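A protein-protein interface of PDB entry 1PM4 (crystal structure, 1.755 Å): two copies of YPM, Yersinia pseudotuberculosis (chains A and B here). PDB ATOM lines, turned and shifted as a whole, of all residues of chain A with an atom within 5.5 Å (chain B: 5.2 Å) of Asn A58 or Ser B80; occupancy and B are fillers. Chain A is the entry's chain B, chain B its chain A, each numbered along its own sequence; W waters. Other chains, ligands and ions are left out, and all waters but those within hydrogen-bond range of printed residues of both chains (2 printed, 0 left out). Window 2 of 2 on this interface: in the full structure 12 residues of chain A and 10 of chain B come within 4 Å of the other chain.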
ATOM      1  N   ASN A  54     -34.667 -11.191   5.130  1.00  0.00           N
ATOM      2  CA  ASN A  54     -33.653 -11.785   4.238  1.00  0.00           C
ATOM      3  C   ASN A  54     -32.489 -10.844   4.083  1.00  0.00           C
ATOM      4  O   ASN A  54     -32.038 -10.580   2.940  1.00  0.00           O
ATOM      5  CB  ASN A  54     -34.195 -12.162   2.848  1.00  0.00           C
ATOM      6  CG  ASN A  54     -34.773 -10.974   2.094  1.00  0.00           C
ATOM      7  OD1 ASN A  54     -35.264 -10.010   2.716  1.00  0.00           O
ATOM      8  ND2 ASN A  54     -34.753 -11.038   0.752  1.00  0.00           N
ATOM      9  N   VAL A  55     -32.040 -10.408   5.244  1.00  0.00           N
ATOM     10  CA  VAL A  55     -30.951  -9.506   5.562  1.00  0.00           C
ATOM     11  C   VAL A  55     -30.674  -8.492   4.502  1.00  0.00           C
ATOM     12  O   VAL A  55     -31.471  -7.542   4.388  1.00  0.00           O
ATOM     13  CB  VAL A  55     -29.756 -10.318   6.048  1.00  0.00           C
ATOM     14  CG1 VAL A  55     -30.192 -10.993   7.271  1.00  0.00           C
ATOM     15  CG2 VAL A  55     -29.301 -11.402   5.002  1.00  0.00           C
ATOM     16  N   GLY A  56     -29.529  -8.640   3.811  1.00  0.00           N
ATOM     17  CA  GLY A  56     -29.365  -8.245   2.416  1.00  0.00           C
ATOM     18  C   GLY A  56     -28.663  -9.320   1.545  1.00  0.00           C
ATOM     19  O   GLY A  56     -27.529  -9.098   1.074  1.00  0.00           O
ATOM     20  N   GLY A  57     -29.299 -10.479   1.324  1.00  0.00           N
ATOM     21  CA  GLY A  57     -28.737 -11.510   0.443  1.00  0.00           C
ATOM     22  C   GLY A  57     -28.211 -12.826   1.030  1.00  0.00           C
ATOM     23  O   GLY A  57     -28.288 -13.858   0.362  1.00  0.00           O
ATOM     24  N   ASN A  58     -27.664 -12.799   2.247  1.00  0.00           N
ATOM     25  CA  ASN A  58     -27.178 -14.007   2.946  1.00  0.00           C
ATOM     26  C   ASN A  58     -28.254 -15.071   3.239  1.00  0.00           C
ATOM     27  O   ASN A  58     -27.930 -16.151   3.732  1.00  0.00           O
ATOM     28  CB  ASN A  58     -26.532 -13.604   4.287  1.00  0.00           C
ATOM     29  CG  ASN A  58     -25.366 -14.559   4.735  1.00  0.00           C
ATOM     30  OD1 ASN A  58     -25.193 -15.657   4.161  1.00  0.00           O
ATOM     31  ND2 ASN A  58     -24.577 -14.138   5.744  1.00  0.00           N
ATOM     32  N   GLY A  59     -29.525 -14.755   2.978  1.00  0.00           N
ATOM     33  CA  GLY A  59     -30.616 -15.611   3.350  1.00  0.00           C
ATOM     34  C   GLY A  59     -31.326 -15.121   4.601  1.00  0.00           C
ATOM     35  O   GLY A  59     -31.086 -14.012   5.121  1.00  0.00           O
ATOM     36  N   TRP A  60     -32.177 -15.992   5.109  1.00  0.00           N
ATOM     37  CA  TRP A  60     -33.122 -15.618   6.132  1.00  0.00           C
ATOM     38  C   TRP A  60     -32.515 -15.668   7.528  1.00  0.00           C
ATOM     39  O   TRP A  60     -31.830 -16.641   7.913  1.00  0.00           O
ATOM     40  CB  TRP A  60     -34.333 -16.524   6.030  1.00  0.00           C
ATOM     41  CG  TRP A  60     -35.085 -16.249   4.760  1.00  0.00           C
ATOM     42  CD1 TRP A  60     -34.970 -16.897   3.566  1.00  0.00           C
ATOM     43  CD2 TRP A  60     -36.058 -15.221   4.563  1.00  0.00           C
ATOM     44  NE1 TRP A  60     -35.800 -16.328   2.635  1.00  0.00           N
ATOM     45  CE2 TRP A  60     -36.491 -15.300   3.223  1.00  0.00           C
ATOM     46  CE3 TRP A  60     -36.608 -14.232   5.386  1.00  0.00           C
ATOM     47  CZ2 TRP A  60     -37.442 -14.447   2.701  1.00  0.00           C
ATOM     48  CZ3 TRP A  60     -37.565 -13.410   4.872  1.00  0.00           C
ATOM     49  CH2 TRP A  60     -37.960 -13.498   3.535  1.00  0.00           C
ATOM     50  N   THR B  29     -21.310 -24.034   7.317  1.00  0.00           N
ATOM     51  CA  THR B  29     -22.681 -23.626   6.987  1.00  0.00           C
ATOM     52  C   THR B  29     -23.685 -24.381   7.867  1.00  0.00           C
ATOM     53  O   THR B  29     -23.596 -25.600   8.038  1.00  0.00           O
ATOM     54  CB  THR B  29     -22.991 -23.862   5.473  1.00  0.00           C
ATOM     55  OG1 THR B  29     -22.352 -22.855   4.679  1.00  0.00           O
ATOM     56  CG2 THR B  29     -24.481 -23.688   5.166  1.00  0.00           C
ATOM     57  N   TYR B  77     -30.812 -18.914   9.058  1.00  0.00           N
ATOM     58  CA  TYR B  77     -30.860 -19.815   7.888  1.00  0.00           C
ATOM     59  C   TYR B  77     -29.936 -19.318   6.785  1.00  0.00           C
ATOM     60  O   TYR B  77     -30.165 -19.546   5.584  1.00  0.00           O
ATOM     61  CB  TYR B  77     -32.285 -19.922   7.356  1.00  0.00           C
ATOM     62  CG  TYR B  77     -33.169 -20.462   8.420  1.00  0.00           C
ATOM     63  CD1 TYR B  77     -33.095 -21.780   8.751  1.00  0.00           C
ATOM     64  CD2 TYR B  77     -33.970 -19.628   9.184  1.00  0.00           C
ATOM     65  CE1 TYR B  77     -33.826 -22.307   9.766  1.00  0.00           C
ATOM     66  CE2 TYR B  77     -34.729 -20.141  10.188  1.00  0.00           C
ATOM     67  CZ  TYR B  77     -34.656 -21.487  10.474  1.00  0.00           C
ATOM     68  OH  TYR B  77     -35.364 -22.058  11.493  1.00  0.00           O
ATOM     69  N   TYR B  78     -28.910 -18.600   7.204  1.00  0.00           N
ATOM     70  CA  TYR B  78     -27.959 -18.006   6.277  1.00  0.00           C
ATOM     71  C   TYR B  78     -27.174 -19.075   5.514  1.00  0.00           C
ATOM     72  O   TYR B  78     -26.856 -20.125   6.056  1.00  0.00           O
ATOM     73  CB  TYR B  78     -26.997 -17.086   7.029  1.00  0.00           C
ATOM     74  CG  TYR B  78     -27.672 -15.907   7.654  1.00  0.00           C
ATOM     75  CD1 TYR B  78     -28.627 -15.177   6.961  1.00  0.00           C
ATOM     76  CD2 TYR B  78     -27.353 -15.504   8.941  1.00  0.00           C
ATOM     77  CE1 TYR B  78     -29.233 -14.075   7.536  1.00  0.00           C
ATOM     78  CE2 TYR B  78     -27.960 -14.413   9.533  1.00  0.00           C
ATOM     79  CZ  TYR B  78     -28.907 -13.704   8.821  1.00  0.00           C
ATOM     80  OH  TYR B  78     -29.528 -12.606   9.399  1.00  0.00           O
ATOM     81  N   THR B  79     -26.870 -18.795   4.253  1.00  0.00           N
ATOM     82  CA  THR B  79     -26.209 -19.807   3.440  1.00  0.00           C
ATOM     83  C   THR B  79     -24.703 -19.863   3.757  1.00  0.00           C
ATOM     84  O   THR B  79     -24.146 -20.962   3.844  1.00  0.00           O
ATOM     85  CB  THR B  79     -26.536 -19.604   1.956  1.00  0.00           C
ATOM     86  OG1 THR B  79     -26.500 -18.212   1.639  1.00  0.00           O
ATOM     87  CG2 THR B  79     -28.002 -20.017   1.714  1.00  0.00           C
ATOM     88  N   SER B  80     -24.074 -18.714   3.974  1.00  0.00           N
ATOM     89  CA  SER B  80     -22.674 -18.686   4.405  1.00  0.00           C
ATOM     90  C   SER B  80     -22.641 -18.961   5.909  1.00  0.00           C
ATOM     91  O   SER B  80     -23.469 -18.463   6.656  1.00  0.00           O
ATOM     92  CB  SER B  80     -21.992 -17.351   4.076  1.00  0.00           C
ATOM     93  OG  SER B  80     -20.582 -17.481   4.101  1.00  0.00           O
ATOM     94  N   GLY B  81     -21.694 -19.783   6.341  1.00  0.00           N
ATOM     95  CA  GLY B  81     -21.587 -20.119   7.749  1.00  0.00           C
ATOM     96  C   GLY B  81     -21.041 -18.941   8.502  1.00  0.00           C
ATOM     97  O   GLY B  81     -20.312 -18.122   7.950  1.00  0.00           O
ATOM     98  N   LEU B  82     -21.387 -18.847   9.776  1.00  0.00           N
ATOM     99  CA  LEU B  82     -20.857 -17.804  10.608  1.00  0.00           C
ATOM    100  C   LEU B  82     -20.751 -18.293  12.023  1.00  0.00           C
ATOM    101  O   LEU B  82     -21.505 -19.166  12.470  1.00  0.00           O
ATOM    102  CB  LEU B  82     -21.742 -16.567  10.556  1.00  0.00           C
ATOM    103  CG  LEU B  82     -21.587 -15.671   9.315  1.00  0.00           C
ATOM    104  CD1 LEU B  82     -22.483 -14.464   9.526  1.00  0.00           C
ATOM    105  CD2 LEU B  82     -20.142 -15.239   9.108  1.00  0.00           C
HETATM  106  O   HOH W   1     -28.607 -17.118   0.246  1.00  0.00           O
HETATM  107  O   HOH W   2     -31.915 -18.662   3.819  1.00  0.00           O
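No position is printed for both chains.
Of the 7 pairs that touch across the chains among the printed residues, none has its exchanged pair printed and touching as well.
OH of Tyr B78 touches CG1 of Val A55, at 2.8 Å.
CA of Tyr B78 touches O of Asn A58, 3.1 Å away.
Gly A59 touches Tyr B78.
Tyr B78 touches Trp A60 (N to O, 3.6 Å).
The backbone NH (N) of Tyr B77 sits at hydrogen-bond distance from the backbone carbonyl oxygen (O) of Trp A60, at 2.7 Å.
The backbone NH of Thr B79 is in hydrogen-bond range of the backbone carbonyl oxygen of Asn A58 (2.9 Å).
The backbone NH (N) of Ser B80 is in hydrogen-bond range of the side-chain amide oxygen (OD1) of Asn A58.
O of Thr B79 is in hydrogen-bond range of OG1 of Thr B29, at 2.7 Å.
Water W2 bridges O of Tyr B77 (2.6 Å) and N of Trp A60 (3.0 Å).
Water W1 bridges OG1 of Thr B79 and O of Gly A57.
Of the 7 printed residues of chain B, 4 touch a printed residue of chain A.
Hydrophobic or aromatic side chains of chain B that line the printed part of chain A: Tyr B77 and Tyr B78.
Along chain B the printed residues that touch a printed residue of chain A span positions 77 to 80.
Of chain B, only Tyr B78, Thr B79 and Ser B80 come within 4 Å of Asn A58.
Of the printed residues of chain B, Gly A59 touches Tyr B78 (3.0 Å).
Of the printed residues of chain A, Tyr B77 touches Trp A60.
Printed residues of chain A within 4 Å of Tyr B78: Val A55 (2.8 Å), Asn A58 (3.1 Å), Gly A59 (3.0 Å) and Trp A60 (3.6 Å).
Of the printed residues of chain A, Thr B79 touches Asn A58 (2.9 Å).
Ser B80 touches just one residue of chain A: Asn A58.
Gly B81 touches none of the printed residues of chain A.
Leu B82 touches none of the printed residues of chain A.
The nearest residue of chain B that does not touch Asn A58 is Leu B82 (4.3 Å).
The nearest printed residue of chain B that does not touch Trp A60 is Thr B79 (6.1 Å).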
